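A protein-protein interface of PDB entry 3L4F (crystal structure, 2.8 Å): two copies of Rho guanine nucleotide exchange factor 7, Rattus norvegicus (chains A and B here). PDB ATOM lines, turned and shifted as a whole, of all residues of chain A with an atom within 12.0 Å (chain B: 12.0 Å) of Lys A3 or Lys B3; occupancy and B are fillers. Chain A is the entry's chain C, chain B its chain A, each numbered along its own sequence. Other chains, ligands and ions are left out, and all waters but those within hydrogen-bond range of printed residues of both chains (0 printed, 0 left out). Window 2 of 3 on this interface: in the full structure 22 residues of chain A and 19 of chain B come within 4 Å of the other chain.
The side-chain hydroxyl (OG1) of Thr B8 is in hydrogen-bond range of the side-chain hydroxyl (OH) of Tyr A10, 3.1 Å away.
OG of Ser A4 is in hydrogen-bond range of N of Val A6, at 2.6 Å. The backbone carbonyl oxygen (O) of Tyr A10 lies close to the side-chain amino group (NZ) of Lys A13, 3.5 Å away.
Among the printed residues, merely in contact across the chains: Lys A3 with Leu B5 (2.9 Å), Ser A4 with Leu B5 (3.4 Å), Leu A12 with Leu B12 (3.4 Å), Val A9 with Thr B8 (3.4 Å), Val A9 with Val B9 (3.5 Å), Tyr A10 with Ser B4 (3.6 Å), Lys A13 with Leu B12 (3.6 Å) and Lys A3 with Lys B3 (3.7 Å).
No residue of chain B comes within 4 Å of Glu A2. Lys A3 touches just these residues of chain B: Lys B3 (3.7 Å) and Leu B5 (2.9 Å). Ser A4 touches just one residue of chain B: Leu B5 (3.4 Å). Val A6 touches none of the printed residues of chain B. Printed residues of chain B within 4 Å of Tyr A10: Ser B4 (3.6 Å) and Thr B8 (3.1 Å). Printed residues of chain B within 4 Å of Leu A12: Leu B12. Of the printed residues of chain B, Lys A13 touches Leu B12. No residue of chain A comes within 4 Å of Glu B2. Of the printed residues of chain A, Lys B3 touches Lys A3 (3.7 Å). Of chain A, only Tyr A10 (3.6 Å) comes within 4 Å of Ser B4. Leu B5 touches just these residues of chain A: Lys A3 (2.9 Å) and Ser A4 (3.4 Å). No residue of chain A comes within 4 Å of Val B6. No residue of chain A comes within 4 Å of Asp B7. Printed residues of chain A within 4 Å of Leu B12: Leu A12 and Lys A13.
Of the 12 printed residues of chain B, 6 touch a printed residue of chain A. Printed residues of chain B that touch a printed residue of chain A: Lys B3, Ser B4, Leu B5, Thr B8, Val B9 and Leu B12. Hydrophobic or aromatic side chains of chain B within 4 Å of the printed part of chain A: Leu B5, Val B9 and Leu B12. Along chain B the printed residues that touch a printed residue of chain A span positions 3 to 12. Among the printed residues, 9 pairs touch across the chains. Among the printed residues, no Asp or Glu carboxylate lies within 4 Å of a Lys or Arg side-chain nitrogen of the other chain.
Lys B3 touches its own counterpart, Lys A3. Ser A4 touches Leu B5, but with the chains exchanged Leu A5 does not touch Ser B4 (11.4 Å). Val A9 touches its own counterpart, Val B9. Leu B12 touches its own counterpart, Leu A12.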
ATOM      1  N   MET A   1      12.767  14.691  23.720  1.00  0.00           N
ATOM      2  CA  MET A   1      14.178  14.323  24.023  1.00  0.00           C
ATOM      3  C   MET A   1      14.607  13.150  23.147  1.00  0.00           C
ATOM      4  O   MET A   1      15.648  12.532  23.374  1.00  0.00           O
ATOM      5  CB  MET A   1      14.320  13.955  25.504  1.00  0.00           C
ATOM      6  CG  MET A   1      15.755  13.745  25.974  1.00  0.00           C
ATOM      7  SD  MET A   1      15.868  13.443  27.754  1.00  0.00           S
ATOM      8  CE  MET A   1      16.078  15.100  28.380  1.00  0.00           C
ATOM      9  N   GLU A   2      13.790  12.845  22.144  1.00  0.00           N
ATOM     10  CA  GLU A   2      14.084  11.755  21.223  1.00  0.00           C
ATOM     11  C   GLU A   2      14.598  12.334  19.912  1.00  0.00           C
ATOM     12  O   GLU A   2      15.477  11.752  19.271  1.00  0.00           O
ATOM     13  CB  GLU A   2      12.831  10.917  20.960  1.00  0.00           C
ATOM     14  CG  GLU A   2      12.293  10.176  22.175  1.00  0.00           C
ATOM     15  CD  GLU A   2      11.828  11.109  23.275  1.00  0.00           C
ATOM     16  OE1 GLU A   2      10.986  11.990  22.998  1.00  0.00           O
ATOM     17  OE2 GLU A   2      12.300  10.958  24.421  1.00  0.00           O
ATOM     18  N   LYS A   3      14.042  13.479  19.519  1.00  0.00           N
ATOM     19  CA  LYS A   3      14.449  14.151  18.287  1.00  0.00           C
ATOM     20  C   LYS A   3      15.940  14.498  18.313  1.00  0.00           C
ATOM     21  O   LYS A   3      16.547  14.581  19.380  1.00  0.00           O
ATOM     22  CB  LYS A   3      13.605  15.419  18.051  1.00  0.00           C
ATOM     23  CG  LYS A   3      13.220  16.213  19.302  1.00  0.00           C
ATOM     24  CD  LYS A   3      12.107  15.526  20.101  1.00  0.00           C
ATOM     25  CE  LYS A   3      11.760  16.289  21.382  1.00  0.00           C
ATOM     26  NZ  LYS A   3      11.204  17.658  21.135  1.00  0.00           N
ATOM     27  N   SER A   4      16.518  14.696  17.130  1.00  0.00           N
ATOM     28  CA  SER A   4      17.944  14.998  16.973  1.00  0.00           C
ATOM     29  C   SER A   4      18.733  13.794  17.486  1.00  0.00           C
ATOM     30  O   SER A   4      18.226  12.672  17.478  1.00  0.00           O
ATOM     31  CB  SER A   4      18.337  16.251  17.760  1.00  0.00           C
ATOM     32  OG  SER A   4      18.746  15.922  19.075  1.00  0.00           O
ATOM     33  N   LEU A   5      19.970  14.019  17.922  1.00  0.00           N
ATOM     34  CA  LEU A   5      20.794  12.935  18.461  1.00  0.00           C
ATOM     35  C   LEU A   5      20.858  13.151  19.974  1.00  0.00           C
ATOM     36  O   LEU A   5      21.347  12.306  20.733  1.00  0.00           O
ATOM     37  CB  LEU A   5      22.188  12.967  17.821  1.00  0.00           C
ATOM     38  CG  LEU A   5      22.145  13.138  16.289  1.00  0.00           C
ATOM     39  CD1 LEU A   5      23.549  13.123  15.703  1.00  0.00           C
ATOM     40  CD2 LEU A   5      21.299  12.033  15.674  1.00  0.00           C
ATOM     41  N   VAL A   6      20.337  14.314  20.372  1.00  0.00           N
ATOM     42  CA  VAL A   6      20.213  14.762  21.758  1.00  0.00           C
ATOM     43  C   VAL A   6      21.479  15.004  22.563  1.00  0.00           C
ATOM     44  O   VAL A   6      21.707  16.113  23.048  1.00  0.00           O
ATOM     45  CB  VAL A   6      19.347  13.798  22.580  1.00  0.00           C
ATOM     46  CG1 VAL A   6      19.049  14.424  23.913  1.00  0.00           C
ATOM     47  CG2 VAL A   6      18.055  13.451  21.828  1.00  0.00           C
ATOM     48  N   ASP A   7      22.289  13.971  22.748  1.00  0.00           N
ATOM     49  CA  ASP A   7      23.499  14.160  23.525  1.00  0.00           C
ATOM     50  C   ASP A   7      24.503  14.975  22.755  1.00  0.00           C
ATOM     51  O   ASP A   7      25.250  15.785  23.325  1.00  0.00           O
ATOM     52  CB  ASP A   7      24.106  12.818  23.941  1.00  0.00           C
ATOM     53  CG  ASP A   7      23.529  12.313  25.247  1.00  0.00           C
ATOM     54  OD1 ASP A   7      23.690  13.025  26.261  1.00  0.00           O
ATOM     55  OD2 ASP A   7      22.908  11.228  25.258  1.00  0.00           O
ATOM     56  N   THR A   8      24.518  14.772  21.448  1.00  0.00           N
ATOM     57  CA  THR A   8      25.439  15.526  20.623  1.00  0.00           C
ATOM     58  C   THR A   8      25.140  17.029  20.771  1.00  0.00           C
ATOM     59  O   THR A   8      26.059  17.852  20.806  1.00  0.00           O
ATOM     60  CB  THR A   8      25.340  15.070  19.151  1.00  0.00           C
ATOM     61  OG1 THR A   8      26.003  13.804  18.993  1.00  0.00           O
ATOM     62  CG2 THR A   8      25.979  16.076  18.245  1.00  0.00           C
ATOM     63  N   VAL A   9      23.860  17.385  20.889  1.00  0.00           N
ATOM     64  CA  VAL A   9      23.492  18.791  21.044  1.00  0.00           C
ATOM     65  C   VAL A   9      24.138  19.437  22.258  1.00  0.00           C
ATOM     66  O   VAL A   9      24.711  20.514  22.160  1.00  0.00           O
ATOM     67  CB  VAL A   9      21.981  18.978  21.159  1.00  0.00           C
ATOM     68  CG1 VAL A   9      21.664  20.382  21.752  1.00  0.00           C
ATOM     69  CG2 VAL A   9      21.357  18.797  19.789  1.00  0.00           C
ATOM     70  N   TYR A  10      24.045  18.785  23.411  1.00  0.00           N
ATOM     71  CA  TYR A  10      24.643  19.346  24.614  1.00  0.00           C
ATOM     72  C   TYR A  10      26.173  19.262  24.562  1.00  0.00           C
ATOM     73  O   TYR A  10      26.865  20.198  24.990  1.00  0.00           O
ATOM     74  CB  TYR A  10      24.051  18.675  25.852  1.00  0.00           C
ATOM     75  CG  TYR A  10      22.630  19.144  26.116  1.00  0.00           C
ATOM     76  CD1 TYR A  10      21.533  18.389  25.700  1.00  0.00           C
ATOM     77  CD2 TYR A  10      22.384  20.390  26.704  1.00  0.00           C
ATOM     78  CE1 TYR A  10      20.228  18.857  25.860  1.00  0.00           C
ATOM     79  CE2 TYR A  10      21.085  20.869  26.866  1.00  0.00           C
ATOM     80  CZ  TYR A  10      20.012  20.098  26.439  1.00  0.00           C
ATOM     81  OH  TYR A  10      18.725  20.578  26.572  1.00  0.00           O
ATOM     82  N   ALA A  11      26.705  18.163  24.028  1.00  0.00           N
ATOM     83  CA  ALA A  11      28.151  18.047  23.866  1.00  0.00           C
ATOM     84  C   ALA A  11      28.610  19.235  23.029  1.00  0.00           C
ATOM     85  O   ALA A  11      29.625  19.841  23.341  1.00  0.00           O
ATOM     86  CB  ALA A  11      28.517  16.755  23.139  1.00  0.00           C
ATOM     87  N   LEU A  12      27.868  19.552  21.958  1.00  0.00           N
ATOM     88  CA  LEU A  12      28.195  20.673  21.064  1.00  0.00           C
ATOM     89  C   LEU A  12      28.060  21.993  21.788  1.00  0.00           C
ATOM     90  O   LEU A  12      28.914  22.876  21.666  1.00  0.00           O
ATOM     91  CB  LEU A  12      27.272  20.697  19.846  1.00  0.00           C
ATOM     92  CG  LEU A  12      27.515  19.643  18.775  1.00  0.00           C
ATOM     93  CD1 LEU A  12      26.503  19.815  17.648  1.00  0.00           C
ATOM     94  CD2 LEU A  12      28.950  19.776  18.275  1.00  0.00           C
ATOM     95  N   LYS A  13      26.966  22.128  22.527  1.00  0.00           N
ATOM     96  CA  LYS A  13      26.725  23.337  23.301  1.00  0.00           C
ATOM     97  C   LYS A  13      27.990  23.557  24.134  1.00  0.00           C
ATOM     98  O   LYS A  13      28.458  24.687  24.312  1.00  0.00           O
ATOM     99  CB  LYS A  13      25.522  23.132  24.228  1.00  0.00           C
ATOM    100  CG  LYS A  13      25.041  24.402  24.926  1.00  0.00           C
ATOM    101  CD  LYS A  13      23.887  24.116  25.900  1.00  0.00           C
ATOM    102  CE  LYS A  13      24.363  23.552  27.257  1.00  0.00           C
ATOM    103  NZ  LYS A  13      25.077  22.230  27.208  1.00  0.00           N
ATOM    104  N   MET B   1       8.841  26.631  17.968  1.00  0.00           N
ATOM    105  CA  MET B   1       9.678  26.281  19.152  1.00  0.00           C
ATOM    106  C   MET B   1       8.848  26.274  20.441  1.00  0.00           C
ATOM    107  O   MET B   1       7.993  27.140  20.640  1.00  0.00           O
ATOM    108  CB  MET B   1      10.821  27.291  19.292  1.00  0.00           C
ATOM    109  CG  MET B   1      11.711  27.425  18.065  1.00  0.00           C
ATOM    110  SD  MET B   1      13.034  28.642  18.289  1.00  0.00           S
ATOM    111  CE  MET B   1      12.155  30.167  17.940  1.00  0.00           C
ATOM    112  N   GLU B   2       9.097  25.289  21.304  1.00  0.00           N
ATOM    113  CA  GLU B   2       8.395  25.178  22.584  1.00  0.00           C
ATOM    114  C   GLU B   2       8.872  23.956  23.383  1.00  0.00           C
ATOM    115  O   GLU B   2       8.243  23.568  24.371  1.00  0.00           O
ATOM    116  CB  GLU B   2       6.863  25.103  22.382  1.00  0.00           C
ATOM    117  CG  GLU B   2       6.053  25.917  23.424  1.00  0.00           C
ATOM    118  CD  GLU B   2       4.542  25.660  23.390  1.00  0.00           C
ATOM    119  OE1 GLU B   2       4.106  24.612  23.916  1.00  0.00           O
ATOM    120  OE2 GLU B   2       3.792  26.502  22.843  1.00  0.00           O
ATOM    121  N   LYS B   3       9.980  23.352  22.950  1.00  0.00           N
ATOM    122  CA  LYS B   3      10.559  22.189  23.637  1.00  0.00           C
ATOM    123  C   LYS B   3      12.014  22.517  24.001  1.00  0.00           C
ATOM    124  O   LYS B   3      12.664  23.329  23.336  1.00  0.00           O
ATOM    125  CB  LYS B   3      10.515  20.933  22.746  1.00  0.00           C
ATOM    126  CG  LYS B   3       9.198  20.702  22.019  1.00  0.00           C
ATOM    127  CD  LYS B   3       9.005  21.736  20.930  1.00  0.00           C
ATOM    128  CE  LYS B   3       7.664  21.603  20.244  1.00  0.00           C
ATOM    129  NZ  LYS B   3       7.467  22.732  19.293  1.00  0.00           N
ATOM    130  N   SER B   4      12.526  21.892  25.055  1.00  0.00           N
ATOM    131  CA  SER B   4      13.893  22.157  25.485  1.00  0.00           C
ATOM    132  C   SER B   4      14.957  21.869  24.410  1.00  0.00           C
ATOM    133  O   SER B   4      15.960  22.584  24.326  1.00  0.00           O
ATOM    134  CB  SER B   4      14.207  21.365  26.764  1.00  0.00           C
ATOM    135  OG  SER B   4      15.433  21.790  27.343  1.00  0.00           O
ATOM    136  N   LEU B   5      14.738  20.845  23.584  1.00  0.00           N
ATOM    137  CA  LEU B   5      15.704  20.494  22.544  1.00  0.00           C
ATOM    138  C   LEU B   5      15.613  21.431  21.351  1.00  0.00           C
ATOM    139  O   LEU B   5      16.607  22.074  21.004  1.00  0.00           O
ATOM    140  CB  LEU B   5      15.485  19.064  22.071  1.00  0.00           C
ATOM    141  CG  LEU B   5      16.576  18.430  21.203  1.00  0.00           C
ATOM    142  CD1 LEU B   5      17.774  18.051  22.056  1.00  0.00           C
ATOM    143  CD2 LEU B   5      15.998  17.200  20.524  1.00  0.00           C
ATOM    144  N   VAL B   6      14.432  21.498  20.727  1.00  0.00           N
ATOM    145  CA  VAL B   6      14.207  22.370  19.569  1.00  0.00           C
ATOM    146  C   VAL B   6      14.832  23.749  19.781  1.00  0.00           C
ATOM    147  O   VAL B   6      15.374  24.333  18.845  1.00  0.00           O
ATOM    148  CB  VAL B   6      12.701  22.578  19.273  1.00  0.00           C
ATOM    149  CG1 VAL B   6      12.524  23.179  17.872  1.00  0.00           C
ATOM    150  CG2 VAL B   6      11.952  21.265  19.405  1.00  0.00           C
ATOM    151  N   ASP B   7      14.752  24.269  21.005  1.00  0.00           N
ATOM    152  CA  ASP B   7      15.341  25.578  21.316  1.00  0.00           C
ATOM    153  C   ASP B   7      16.836  25.529  21.615  1.00  0.00           C
ATOM    154  O   ASP B   7      17.565  26.430  21.208  1.00  0.00           O
ATOM    155  CB  ASP B   7      14.627  26.256  22.490  1.00  0.00           C
ATOM    156  CG  ASP B   7      13.242  26.728  22.123  1.00  0.00           C
ATOM    157  OD1 ASP B   7      13.039  27.103  20.949  1.00  0.00           O
ATOM    158  OD2 ASP B   7      12.359  26.740  23.008  1.00  0.00           O
ATOM    159  N   THR B   8      17.292  24.502  22.336  1.00  0.00           N
ATOM    160  CA  THR B   8      18.718  24.377  22.632  1.00  0.00           C
ATOM    161  C   THR B   8      19.444  24.424  21.286  1.00  0.00           C
ATOM    162  O   THR B   8      20.506  25.048  21.148  1.00  0.00           O
ATOM    163  CB  THR B   8      19.049  23.031  23.301  1.00  0.00           C
ATOM    164  OG1 THR B   8      18.256  22.862  24.480  1.00  0.00           O
ATOM    165  CG2 THR B   8      20.503  22.982  23.681  1.00  0.00           C
ATOM    166  N   VAL B   9      18.842  23.767  20.292  1.00  0.00           N
ATOM    167  CA  VAL B   9      19.406  23.700  18.947  1.00  0.00           C
ATOM    168  C   VAL B   9      19.376  25.041  18.210  1.00  0.00           C
ATOM    169  O   VAL B   9      20.384  25.447  17.612  1.00  0.00           O
ATOM    170  CB  VAL B   9      18.705  22.583  18.101  1.00  0.00           C
ATOM    171  CG1 VAL B   9      19.016  22.730  16.614  1.00  0.00           C
ATOM    172  CG2 VAL B   9      19.208  21.234  18.558  1.00  0.00           C
ATOM    173  N   TYR B  10      18.251  25.746  18.247  1.00  0.00           N
ATOM    174  CA  TYR B  10      18.231  27.024  17.555  1.00  0.00           C
ATOM    175  C   TYR B  10      19.076  28.086  18.247  1.00  0.00           C
ATOM    176  O   TYR B  10      19.375  29.134  17.664  1.00  0.00           O
ATOM    177  CB  TYR B  10      16.802  27.508  17.305  1.00  0.00           C
ATOM    178  CG  TYR B  10      16.290  26.939  16.004  1.00  0.00           C
ATOM    179  CD1 TYR B  10      15.870  25.611  15.924  1.00  0.00           C
ATOM    180  CD2 TYR B  10      16.359  27.680  14.821  1.00  0.00           C
ATOM    181  CE1 TYR B  10      15.543  25.024  14.699  1.00  0.00           C
ATOM    182  CE2 TYR B  10      16.034  27.104  13.587  1.00  0.00           C
ATOM    183  CZ  TYR B  10      15.629  25.770  13.530  1.00  0.00           C
ATOM    184  OH  TYR B  10      15.352  25.161  12.312  1.00  0.00           O
ATOM    185  N   ALA B  11      19.491  27.795  19.475  1.00  0.00           N
ATOM    186  CA  ALA B  11      20.348  28.709  20.217  1.00  0.00           C
ATOM    187  C   ALA B  11      21.764  28.484  19.687  1.00  0.00           C
ATOM    188  O   ALA B  11      22.373  29.399  19.136  1.00  0.00           O
ATOM    189  CB  ALA B  11      20.281  28.411  21.712  1.00  0.00           C
ATOM    190  N   LEU B  12      22.283  27.265  19.846  1.00  0.00           N
ATOM    191  CA  LEU B  12      23.615  26.934  19.330  1.00  0.00           C
ATOM    192  C   LEU B  12      23.737  27.406  17.862  1.00  0.00           C
ATOM    193  O   LEU B  12      24.739  28.021  17.467  1.00  0.00           O
ATOM    194  CB  LEU B  12      23.847  25.428  19.398  1.00  0.00           C
ATOM    195  CG  LEU B  12      25.140  24.920  20.048  1.00  0.00           C
ATOM    196  CD1 LEU B  12      25.487  23.542  19.511  1.00  0.00           C
ATOM    197  CD2 LEU B  12      26.276  25.882  19.751  1.00  0.00           C
